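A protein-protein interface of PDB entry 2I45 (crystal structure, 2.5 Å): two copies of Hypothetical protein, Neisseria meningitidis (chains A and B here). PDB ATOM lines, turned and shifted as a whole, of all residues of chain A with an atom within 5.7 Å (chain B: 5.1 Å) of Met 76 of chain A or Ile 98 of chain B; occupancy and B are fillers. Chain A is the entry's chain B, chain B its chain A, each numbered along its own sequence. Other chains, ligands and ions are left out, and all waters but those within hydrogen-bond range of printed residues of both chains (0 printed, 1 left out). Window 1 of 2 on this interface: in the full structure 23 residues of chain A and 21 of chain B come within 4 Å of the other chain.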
ATOM      1  N   PHE A  29     -41.666   4.450   2.205  1.00  0.00           N
ATOM      2  CA  PHE A  29     -40.505   4.310   1.320  1.00  0.00           C
ATOM      3  C   PHE A  29     -40.771   3.516   0.067  1.00  0.00           C
ATOM      4  O   PHE A  29     -41.502   2.516   0.103  1.00  0.00           O
ATOM      5  CB  PHE A  29     -39.344   3.671   2.038  1.00  0.00           C
ATOM      6  CG  PHE A  29     -38.688   4.568   3.016  1.00  0.00           C
ATOM      7  CD1 PHE A  29     -37.923   5.648   2.577  1.00  0.00           C
ATOM      8  CD2 PHE A  29     -38.817   4.329   4.383  1.00  0.00           C
ATOM      9  CE1 PHE A  29     -37.301   6.510   3.498  1.00  0.00           C
ATOM     10  CE2 PHE A  29     -38.184   5.145   5.321  1.00  0.00           C
ATOM     11  CZ  PHE A  29     -37.432   6.250   4.890  1.00  0.00           C
ATOM     12  N   VAL A  51     -31.732   8.143  -2.769  1.00  0.00           N
ATOM     13  CA  VAL A  51     -30.478   7.709  -2.225  1.00  0.00           C
ATOM     14  C   VAL A  51     -30.152   6.627  -3.194  1.00  0.00           C
ATOM     15  O   VAL A  51     -31.077   6.033  -3.692  1.00  0.00           O
ATOM     16  CB  VAL A  51     -30.630   7.134  -0.842  1.00  0.00           C
ATOM     17  CG1 VAL A  51     -29.300   6.500  -0.409  1.00  0.00           C
ATOM     18  CG2 VAL A  51     -31.144   8.241   0.188  1.00  0.00           C
ATOM     19  N   LEU A  52     -28.864   6.393  -3.495  1.00  0.00           N
ATOM     20  CA  LEU A  52     -28.455   5.425  -4.485  1.00  0.00           C
ATOM     21  C   LEU A  52     -27.461   4.544  -3.832  1.00  0.00           C
ATOM     22  O   LEU A  52     -26.519   5.020  -3.194  1.00  0.00           O
ATOM     23  CB  LEU A  52     -27.733   6.072  -5.680  1.00  0.00           C
ATOM     24  CG  LEU A  52     -28.181   7.174  -6.696  1.00  0.00           C
ATOM     25  CD1 LEU A  52     -27.914   6.746  -8.183  1.00  0.00           C
ATOM     26  CD2 LEU A  52     -29.595   7.596  -6.512  1.00  0.00           C
ATOM     27  N   PHE A  53     -27.617   3.236  -3.972  1.00  0.00           N
ATOM     28  CA  PHE A  53     -26.678   2.425  -3.291  1.00  0.00           C
ATOM     29  C   PHE A  53     -26.151   1.376  -4.270  1.00  0.00           C
ATOM     30  O   PHE A  53     -26.917   0.671  -4.914  1.00  0.00           O
ATOM     31  CB  PHE A  53     -27.268   1.902  -1.968  1.00  0.00           C
ATOM     32  CG  PHE A  53     -26.490   0.746  -1.361  1.00  0.00           C
ATOM     33  CD1 PHE A  53     -25.140   0.863  -1.084  1.00  0.00           C
ATOM     34  CD2 PHE A  53     -27.131  -0.450  -1.052  1.00  0.00           C
ATOM     35  CE1 PHE A  53     -24.384  -0.200  -0.514  1.00  0.00           C
ATOM     36  CE2 PHE A  53     -26.424  -1.514  -0.510  1.00  0.00           C
ATOM     37  CZ  PHE A  53     -25.010  -1.396  -0.240  1.00  0.00           C
ATOM     38  N   ALA A  54     -24.834   1.307  -4.408  1.00  0.00           N
ATOM     39  CA  ALA A  54     -24.281   0.506  -5.468  1.00  0.00           C
ATOM     40  C   ALA A  54     -24.082  -0.791  -4.852  1.00  0.00           C
ATOM     41  O   ALA A  54     -22.975  -1.071  -4.248  1.00  0.00           O
ATOM     42  CB  ALA A  54     -22.982   1.039  -5.927  1.00  0.00           C
ATOM     43  N   ILE A  71     -19.753   6.226  -7.791  1.00  0.00           N
ATOM     44  CA  ILE A  71     -20.340   5.393  -6.746  1.00  0.00           C
ATOM     45  C   ILE A  71     -19.869   3.949  -6.953  1.00  0.00           C
ATOM     46  O   ILE A  71     -20.330   3.292  -7.912  1.00  0.00           O
ATOM     47  CB  ILE A  71     -21.870   5.458  -6.772  1.00  0.00           C
ATOM     48  CG1 ILE A  71     -22.335   6.911  -6.841  1.00  0.00           C
ATOM     49  CG2 ILE A  71     -22.434   4.721  -5.532  1.00  0.00           C
ATOM     50  CD1 ILE A  71     -23.856   7.100  -6.885  1.00  0.00           C
ATOM     51  N   GLY A  74     -20.580  -0.641  -2.948  1.00  0.00           N
ATOM     52  CA  GLY A  74     -20.531  -0.607  -1.478  1.00  0.00           C
ATOM     53  C   GLY A  74     -20.820   0.797  -0.985  1.00  0.00           C
ATOM     54  O   GLY A  74     -20.709   1.032   0.215  1.00  0.00           O
ATOM     55  N   GLU A  75     -21.142   1.726  -1.896  1.00  0.00           N
ATOM     56  CA  GLU A  75     -21.175   3.090  -1.511  1.00  0.00           C
ATOM     57  C   GLU A  75     -22.553   3.708  -1.741  1.00  0.00           C
ATOM     58  O   GLU A  75     -23.274   3.321  -2.687  1.00  0.00           O
ATOM     59  CB  GLU A  75     -20.127   3.876  -2.277  1.00  0.00           C
ATOM     60  CG  GLU A  75     -18.678   3.429  -2.113  1.00  0.00           C
ATOM     61  CD  GLU A  75     -17.645   4.379  -2.778  1.00  0.00           C
ATOM     62  OE1 GLU A  75     -17.890   4.985  -3.830  1.00  0.00           O
ATOM     63  OE2 GLU A  75     -16.551   4.516  -2.249  1.00  0.00           O
ATOM     64  N   MET A  76     -22.916   4.653  -0.881  1.00  0.00           N
ATOM     65  CA  MET A  76     -24.150   5.395  -1.109  1.00  0.00           C
ATOM     66  C   MET A  76     -23.885   6.832  -1.491  1.00  0.00           C
ATOM     67  O   MET A  76     -22.841   7.377  -1.180  1.00  0.00           O
ATOM     68  CB  MET A  76     -25.007   5.424   0.121  1.00  0.00           C
ATOM     69  CG  MET A  76     -25.868   4.251   0.233  1.00  0.00           C
ATOM     70  SD  MET A  76     -26.651   4.031   2.077  1.00  0.00           S
ATOM     71  CE  MET A  76     -27.372   2.208   1.714  1.00  0.00           C
ATOM     72  N   ALA A  77     -24.843   7.443  -2.153  1.00  0.00           N
ATOM     73  CA  ALA A  77     -24.807   8.850  -2.450  1.00  0.00           C
ATOM     74  C   ALA A  77     -26.251   9.313  -2.614  1.00  0.00           C
ATOM     75  O   ALA A  77     -27.155   8.512  -2.541  1.00  0.00           O
ATOM     76  CB  ALA A  77     -24.029   9.094  -3.706  1.00  0.00           C
ATOM     77  N   VAL A  78     -26.487  10.606  -2.812  1.00  0.00           N
ATOM     78  CA  VAL A  78     -27.848  11.022  -2.975  1.00  0.00           C
ATOM     79  C   VAL A  78     -28.047  11.948  -4.173  1.00  0.00           C
ATOM     80  O   VAL A  78     -27.280  12.864  -4.384  1.00  0.00           O
ATOM     81  CB  VAL A  78     -28.462  11.533  -1.643  1.00  0.00           C
ATOM     82  CG1 VAL A  78     -27.398  11.674  -0.584  1.00  0.00           C
ATOM     83  CG2 VAL A  78     -29.297  12.814  -1.825  1.00  0.00           C
ATOM     84  N   ILE A  98     -33.735   4.842  -3.266  1.00  0.00           N
ATOM     85  CA  ILE A  98     -34.698   4.994  -2.179  1.00  0.00           C
ATOM     86  C   ILE A  98     -35.375   6.384  -2.139  1.00  0.00           C
ATOM     87  O   ILE A  98     -34.727   7.405  -2.271  1.00  0.00           O
ATOM     88  CB  ILE A  98     -34.050   4.685  -0.787  1.00  0.00           C
ATOM     89  CG1 ILE A  98     -33.525   3.270  -0.757  1.00  0.00           C
ATOM     90  CG2 ILE A  98     -35.025   4.815   0.317  1.00  0.00           C
ATOM     91  CD1 ILE A  98     -32.022   3.154  -0.740  1.00  0.00           C
ATOM     92  N   GLU B   4     -20.920  13.936  -3.167  1.00  0.00           N
ATOM     93  CA  GLU B   4     -20.317  13.345  -1.927  1.00  0.00           C
ATOM     94  C   GLU B   4     -20.808  11.936  -1.500  1.00  0.00           C
ATOM     95  O   GLU B   4     -21.591  11.786  -0.547  1.00  0.00           O
ATOM     96  CB  GLU B   4     -20.446  14.340  -0.762  1.00  0.00           C
ATOM     97  CG  GLU B   4     -19.226  15.201  -0.524  1.00  0.00           C
ATOM     98  CD  GLU B   4     -17.985  14.352  -0.307  1.00  0.00           C
ATOM     99  OE1 GLU B   4     -17.484  14.314   0.848  1.00  0.00           O
ATOM    100  OE2 GLU B   4     -17.534  13.706  -1.289  1.00  0.00           O
ATOM    101  N   THR B   5     -20.316  10.906  -2.190  1.00  0.00           N
ATOM    102  CA  THR B   5     -20.666   9.513  -1.851  1.00  0.00           C
ATOM    103  C   THR B   5     -20.033   9.141  -0.540  1.00  0.00           C
ATOM    104  O   THR B   5     -18.940   9.616  -0.248  1.00  0.00           O
ATOM    105  CB  THR B   5     -20.188   8.483  -2.898  1.00  0.00           C
ATOM    106  OG1 THR B   5     -18.812   8.193  -2.678  1.00  0.00           O
ATOM    107  CG2 THR B   5     -20.356   9.030  -4.280  1.00  0.00           C
ATOM    108  N   ILE B   6     -20.735   8.282   0.199  1.00  0.00           N
ATOM    109  CA  ILE B   6     -20.353   7.759   1.499  1.00  0.00           C
ATOM    110  C   ILE B   6     -19.886   6.309   1.376  1.00  0.00           C
ATOM    111  O   ILE B   6     -20.719   5.417   1.109  1.00  0.00           O
ATOM    112  CB  ILE B   6     -21.591   7.716   2.442  1.00  0.00           C
ATOM    113  CG1 ILE B   6     -22.136   9.096   2.744  1.00  0.00           C
ATOM    114  CG2 ILE B   6     -21.296   6.971   3.727  1.00  0.00           C
ATOM    115  CD1 ILE B   6     -23.628   9.041   2.959  1.00  0.00           C
ATOM    116  N   LEU B   8     -19.435   3.081   2.808  1.00  0.00           N
ATOM    117  CA  LEU B   8     -19.938   2.368   3.958  1.00  0.00           C
ATOM    118  C   LEU B   8     -18.811   1.555   4.661  1.00  0.00           C
ATOM    119  O   LEU B   8     -18.509   1.827   5.809  1.00  0.00           O
ATOM    120  CB  LEU B   8     -21.181   1.556   3.545  1.00  0.00           C
ATOM    121  CG  LEU B   8     -22.583   2.239   3.663  1.00  0.00           C
ATOM    122  CD1 LEU B   8     -22.632   3.780   3.707  1.00  0.00           C
ATOM    123  CD2 LEU B   8     -23.697   1.704   2.737  1.00  0.00           C
ATOM    124  N   PHE B  29     -31.736  13.784   3.517  1.00  0.00           N
ATOM    125  CA  PHE B  29     -31.414  12.540   4.229  1.00  0.00           C
ATOM    126  C   PHE B  29     -30.354  12.612   5.336  1.00  0.00           C
ATOM    127  O   PHE B  29     -29.254  13.144   5.121  1.00  0.00           O
ATOM    128  CB  PHE B  29     -30.986  11.470   3.213  1.00  0.00           C
ATOM    129  CG  PHE B  29     -32.039  11.164   2.201  1.00  0.00           C
ATOM    130  CD1 PHE B  29     -33.092  10.314   2.504  1.00  0.00           C
ATOM    131  CD2 PHE B  29     -32.008  11.753   0.946  1.00  0.00           C
ATOM    132  CE1 PHE B  29     -34.097  10.045   1.543  1.00  0.00           C
ATOM    133  CE2 PHE B  29     -32.998  11.484  -0.015  1.00  0.00           C
ATOM    134  CZ  PHE B  29     -34.045  10.639   0.285  1.00  0.00           C
ATOM    135  N   GLN B  30     -30.712  12.043   6.502  1.00  0.00           N
ATOM    136  CA  GLN B  30     -29.824  11.779   7.631  1.00  0.00           C
ATOM    137  C   GLN B  30     -29.412  10.302   7.571  1.00  0.00           C
ATOM    138  O   GLN B  30     -30.279   9.420   7.553  1.00  0.00           O
ATOM    139  CB  GLN B  30     -30.592  11.983   8.930  1.00  0.00           C
ATOM    140  CG  GLN B  30     -29.945  12.991   9.889  1.00  0.00           C
ATOM    141  CD  GLN B  30     -30.287  12.773  11.362  1.00  0.00           C
ATOM    142  OE1 GLN B  30     -30.644  11.669  11.782  1.00  0.00           O
ATOM    143  NE2 GLN B  30     -30.157  13.827  12.157  1.00  0.00           N
ATOM    144  N   PHE B  31     -28.114  10.009   7.561  1.00  0.00           N
ATOM    145  CA  PHE B  31     -27.647   8.608   7.675  1.00  0.00           C
ATOM    146  C   PHE B  31     -27.070   8.359   9.059  1.00  0.00           C
ATOM    147  O   PHE B  31     -26.381   9.222   9.573  1.00  0.00           O
ATOM    148  CB  PHE B  31     -26.580   8.325   6.645  1.00  0.00           C
ATOM    149  CG  PHE B  31     -27.032   8.498   5.246  1.00  0.00           C
ATOM    150  CD1 PHE B  31     -27.344   7.398   4.483  1.00  0.00           C
ATOM    151  CD2 PHE B  31     -27.096   9.779   4.666  1.00  0.00           C
ATOM    152  CE1 PHE B  31     -27.756   7.551   3.160  1.00  0.00           C
ATOM    153  CE2 PHE B  31     -27.535   9.977   3.360  1.00  0.00           C
ATOM    154  CZ  PHE B  31     -27.867   8.873   2.593  1.00  0.00           C
ATOM    155  N   HIS B  32     -27.361   7.204   9.670  1.00  0.00           N
ATOM    156  CA  HIS B  32     -26.673   6.776  10.920  1.00  0.00           C
ATOM    157  C   HIS B  32     -25.948   5.503  10.677  1.00  0.00           C
ATOM    158  O   HIS B  32     -26.513   4.569  10.174  1.00  0.00           O
ATOM    159  CB  HIS B  32     -27.650   6.493  12.021  1.00  0.00           C
ATOM    160  CG  HIS B  32     -28.431   7.682  12.433  1.00  0.00           C
ATOM    161  ND1 HIS B  32     -28.216   8.332  13.632  1.00  0.00           N
ATOM    162  CD2 HIS B  32     -29.411   8.367  11.796  1.00  0.00           C
ATOM    163  CE1 HIS B  32     -29.037   9.365  13.716  1.00  0.00           C
ATOM    164  NE2 HIS B  32     -29.772   9.410  12.614  1.00  0.00           N
ATOM    165  N   ASP B  49     -40.236   7.487   9.082  1.00  0.00           N
ATOM    166  CA  ASP B  49     -39.840   6.112   8.839  1.00  0.00           C
ATOM    167  C   ASP B  49     -38.365   5.993   8.683  1.00  0.00           C
ATOM    168  O   ASP B  49     -37.674   6.930   8.309  1.00  0.00           O
ATOM    169  CB  ASP B  49     -40.490   5.578   7.578  1.00  0.00           C
ATOM    170  CG  ASP B  49     -41.953   5.355   7.745  1.00  0.00           C
ATOM    171  OD1 ASP B  49     -42.651   5.187   6.725  1.00  0.00           O
ATOM    172  OD2 ASP B  49     -42.418   5.388   8.892  1.00  0.00           O
ATOM    173  N   LYS B  50     -37.866   4.809   8.937  1.00  0.00           N
ATOM    174  CA  LYS B  50     -36.453   4.603   8.815  1.00  0.00           C
ATOM    175  C   LYS B  50     -36.140   3.377   7.992  1.00  0.00           C
ATOM    176  O   LYS B  50     -36.906   2.414   7.957  1.00  0.00           O
ATOM    177  CB  LYS B  50     -35.835   4.496  10.193  1.00  0.00           C
ATOM    178  CG  LYS B  50     -35.824   5.846  10.930  1.00  0.00           C
ATOM    179  CD  LYS B  50     -34.855   5.686  12.159  1.00  0.00           C
ATOM    180  CE  LYS B  50     -35.015   6.963  13.069  1.00  0.00           C
ATOM    181  NZ  LYS B  50     -34.035   6.765  14.242  1.00  0.00           N
ATOM    182  N   VAL B  51     -34.980   3.436   7.345  1.00  0.00           N
ATOM    183  CA  VAL B  51     -34.482   2.354   6.572  1.00  0.00           C
ATOM    184  C   VAL B  51     -33.259   1.782   7.309  1.00  0.00           C
ATOM    185  O   VAL B  51     -32.261   2.467   7.596  1.00  0.00           O
ATOM    186  CB  VAL B  51     -34.111   2.796   5.118  1.00  0.00           C
ATOM    187  CG1 VAL B  51     -34.009   1.601   4.260  1.00  0.00           C
ATOM    188  CG2 VAL B  51     -35.154   3.779   4.483  1.00  0.00           C
ATOM    189  N   LEU B  52     -33.346   0.513   7.651  1.00  0.00           N
ATOM    190  CA  LEU B  52     -32.215  -0.085   8.295  1.00  0.00           C
ATOM    191  C   LEU B  52     -31.610  -1.056   7.326  1.00  0.00           C
ATOM    192  O   LEU B  52     -32.321  -1.867   6.737  1.00  0.00           O
ATOM    193  CB  LEU B  52     -32.629  -0.838   9.555  1.00  0.00           C
ATOM    194  CG  LEU B  52     -33.547  -0.273  10.656  1.00  0.00           C
ATOM    195  CD1 LEU B  52     -33.086  -0.817  12.023  1.00  0.00           C
ATOM    196  CD2 LEU B  52     -33.656   1.235  10.674  1.00  0.00           C
ATOM    197  N   PHE B  53     -30.306  -0.981   7.150  1.00  0.00           N
ATOM    198  CA  PHE B  53     -29.674  -1.820   6.145  1.00  0.00           C
ATOM    199  C   PHE B  53     -28.530  -2.495   6.863  1.00  0.00           C
ATOM    200  O   PHE B  53     -27.684  -1.873   7.458  1.00  0.00           O
ATOM    201  CB  PHE B  53     -29.251  -1.018   4.864  1.00  0.00           C
ATOM    202  CG  PHE B  53     -28.305  -1.770   3.965  1.00  0.00           C
ATOM    203  CD1 PHE B  53     -28.584  -3.083   3.571  1.00  0.00           C
ATOM    204  CD2 PHE B  53     -27.095  -1.185   3.536  1.00  0.00           C
ATOM    205  CE1 PHE B  53     -27.700  -3.831   2.774  1.00  0.00           C
ATOM    206  CE2 PHE B  53     -26.119  -1.942   2.752  1.00  0.00           C
ATOM    207  CZ  PHE B  53     -26.446  -3.268   2.354  1.00  0.00           C
ATOM    208  N   MET B  76     -32.650  -5.384   4.061  1.00  0.00           N
ATOM    209  CA  MET B  76     -32.991  -4.004   4.254  1.00  0.00           C
ATOM    210  C   MET B  76     -34.433  -4.022   4.702  1.00  0.00           C
ATOM    211  O   MET B  76     -35.231  -4.789   4.177  1.00  0.00           O
ATOM    212  CB  MET B  76     -32.793  -3.286   2.914  1.00  0.00           C
ATOM    213  CG  MET B  76     -33.398  -1.912   2.728  1.00  0.00           C
ATOM    214  SD  MET B  76     -32.469  -0.850   1.247  1.00  0.00           S
ATOM    215  CE  MET B  76     -30.597  -1.185   1.816  1.00  0.00           C
ATOM    216  N   VAL B  96     -26.508   0.723   8.680  1.00  0.00           N
ATOM    217  CA  VAL B  96     -26.723   2.029   8.178  1.00  0.00           C
ATOM    218  C   VAL B  96     -28.238   2.290   8.267  1.00  0.00           C
ATOM    219  O   VAL B  96     -29.062   1.464   7.838  1.00  0.00           O
ATOM    220  CB  VAL B  96     -26.218   2.167   6.706  1.00  0.00           C
ATOM    221  CG1 VAL B  96     -26.646   3.503   6.081  1.00  0.00           C
ATOM    222  CG2 VAL B  96     -24.717   2.038   6.641  1.00  0.00           C
ATOM    223  N   LEU B  97     -28.578   3.472   8.751  1.00  0.00           N
ATOM    224  CA  LEU B  97     -29.946   3.858   8.987  1.00  0.00           C
ATOM    225  C   LEU B  97     -30.231   5.137   8.270  1.00  0.00           C
ATOM    226  O   LEU B  97     -29.565   6.140   8.502  1.00  0.00           O
ATOM    227  CB  LEU B  97     -30.103   4.114  10.466  1.00  0.00           C
ATOM    228  CG  LEU B  97     -31.447   3.692  11.039  1.00  0.00           C
ATOM    229  CD1 LEU B  97     -31.328   3.186  12.475  1.00  0.00           C
ATOM    230  CD2 LEU B  97     -32.432   4.879  10.950  1.00  0.00           C
ATOM    231  N   ILE B  98     -31.213   5.116   7.390  1.00  0.00           N
ATOM    232  CA  ILE B  98     -31.539   6.280   6.613  1.00  0.00           C
ATOM    233  C   ILE B  98     -32.869   6.953   7.109  1.00  0.00           C
ATOM    234  O   ILE B  98     -33.895   6.281   7.246  1.00  0.00           O
ATOM    235  CB  ILE B  98     -31.577   5.892   5.145  1.00  0.00           C
ATOM    236  CG1 ILE B  98     -30.332   5.089   4.800  1.00  0.00           C
ATOM    237  CG2 ILE B  98     -31.712   7.103   4.249  1.00  0.00           C
ATOM    238  CD1 ILE B  98     -30.386   4.500   3.429  1.00  0.00           C
ATOM    239  N   GLU B  99     -32.802   8.266   7.376  1.00  0.00           N
ATOM    240  CA  GLU B  99     -33.900   9.127   7.954  1.00  0.00           C
ATOM    241  C   GLU B  99     -34.155  10.303   7.085  1.00  0.00           C
ATOM    242  O   GLU B  99     -33.375  10.601   6.193  1.00  0.00           O
ATOM    243  CB  GLU B  99     -33.462   9.800   9.265  1.00  0.00           C
ATOM    244  CG  GLU B  99     -33.908   9.135  10.556  1.00  0.00           C
ATOM    245  CD  GLU B  99     -33.534   9.946  11.808  1.00  0.00           C
ATOM    246  OE1 GLU B  99     -34.051  11.118  12.010  1.00  0.00           O
ATOM    247  OE2 GLU B  99     -32.738   9.400  12.600  1.00  0.00           O
ATOM    248  N   LEU B 100     -35.197  11.054   7.441  1.00  0.00           N
ATOM    249  CA  LEU B 100     -35.506  12.289   6.780  1.00  0.00           C
ATOM    250  C   LEU B 100     -35.077  13.564   7.575  1.00  0.00           C
ATOM    251  O   LEU B 100     -33.943  13.596   8.109  1.00  0.00           O
ATOM    252  CB  LEU B 100     -36.974  12.265   6.381  1.00  0.00           C
ATOM    253  CG  LEU B 100     -37.195  12.839   4.975  1.00  0.00           C
ATOM    254  CD1 LEU B 100     -37.056  11.750   3.876  1.00  0.00           C
ATOM    255  CD2 LEU B 100     -38.541  13.616   4.904  1.00  0.00           C
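N of Ile 6 of chain B is in hydrogen-bond range of O of Met 76 of chain A.
NZ of Lys 50 of chain B is in salt-bridge range of OE2 of Glu 99 of chain B, at 3.4 Å. N of Ile 98 of chain B sits at hydrogen-bond distance from O of Val 51 of chain B, 2.9 Å away. O of Val 96 of chain B sits at hydrogen-bond distance from N of Phe 53 of chain B (2.8 Å). The backbone carbonyl oxygen of Val 51 of chain A is in hydrogen-bond range of the backbone NH of Ile 98 of chain A, at 2.9 Å. The backbone carbonyl oxygen (O) of Ala 54 of chain A is in hydrogen-bond range of the backbone NH (N) of Gly 74 of chain A, at 2.8 Å. N of Ala 54 of chain A is in hydrogen-bond range of O of Glu 75 of chain A (3.1 Å).
Among the printed residues, merely in contact across the chains: Met 76 of chain A with Thr 5 of chain B (3.1 Å), Phe 53 of chain A with Phe 53 of chain B (3.2 Å), Phe 29 of chain A with Asp 49 of chain B (3.3 Å), Phe 29 of chain A with Val 51 of chain B (3.4 Å), Gly 74 of chain A with Leu 8 of chain B (3.4 Å), Glu 75 of chain A with Thr 5 of chain B (3.5 Å), Glu 75 of chain A with Ile 6 of chain B (3.5 Å), Phe 29 of chain A with Lys 50 of chain B (3.6 Å), Val 51 of chain A with Phe 29 of chain B (3.7 Å), Ala 77 of chain A with Thr 5 of chain B (3.7 Å), Met 76 of chain A with Leu 8 of chain B (3.8 Å), Phe 53 of chain A with Leu 8 of chain B (3.8 Å), Met 76 of chain A with Phe 31 of chain B (3.8 Å), Met 76 of chain A with Phe 53 of chain B (3.9 Å), Ile 71 of chain A with Thr 5 of chain B (3.9 Å) and Met 76 of chain A with Ile 98 of chain B (3.9998 Å).
Of the printed residues of chain B, Phe 29 of chain A touches Asp 49 (3.3 Å), Lys 50 (3.6 Å) and Val 51 (3.4 Å). Of the printed residues of chain B, Phe 53 of chain A touches Leu 8 (3.8 Å) and Phe 53 (3.2 Å). Printed residues of chain B within 4 Å of Met 76 of chain A: Thr 5, Ile 6, Leu 8, Phe 31, Phe 53 and Ile 98. Of the printed residues of chain B, Ala 77 of chain A touches Thr 5. Printed residues of chain A within 4 Å of Ile 6 of chain B: Glu 75 and Met 76. Printed residues of chain A within 4 Å of Phe 31 of chain B: Met 76 (3.8 Å). Of the printed residues of chain A, Ile 98 of chain B touches Met 76 (3.9998 Å).
Of the 19 printed residues of chain B, 10 touch a printed residue of chain A. Hydrophobic or aromatic side chains of chain B that line the printed part of chain A: Ile 6, Leu 8, Phe 29, Phe 31, Val 51, Phe 53 and Ile 98. Among the printed residues, 17 pairs touch across the chains. Among the printed residues, no Asp or Glu carboxylate lies within 4 Å of a Lys or Arg side-chain nitrogen of the other chain.
Phe 29 of chain A touches Val 51 of chain B, and with the chains exchanged Val 51 of chain A touches Phe 29 of chain B. Phe 53 of chain B touches its own counterpart, Phe 53 of chain A. Met 76 of chain A touches Phe 53 of chain B, but with the chains exchanged Phe 53 of chain A does not touch Met 76 of chain B (4.6 Å). Met 76 of chain A touches Ile 98 of chain B, but with the chains exchanged Ile 98 of chain A does not touch Met 76 of chain B (4.5 Å). Positions printed for both chains: 29, 51, 52, 53, 76 and 98. Of the 17 pairs that touch across the chains among the printed residues, 3 have their exchanged pair printed and touching as well.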
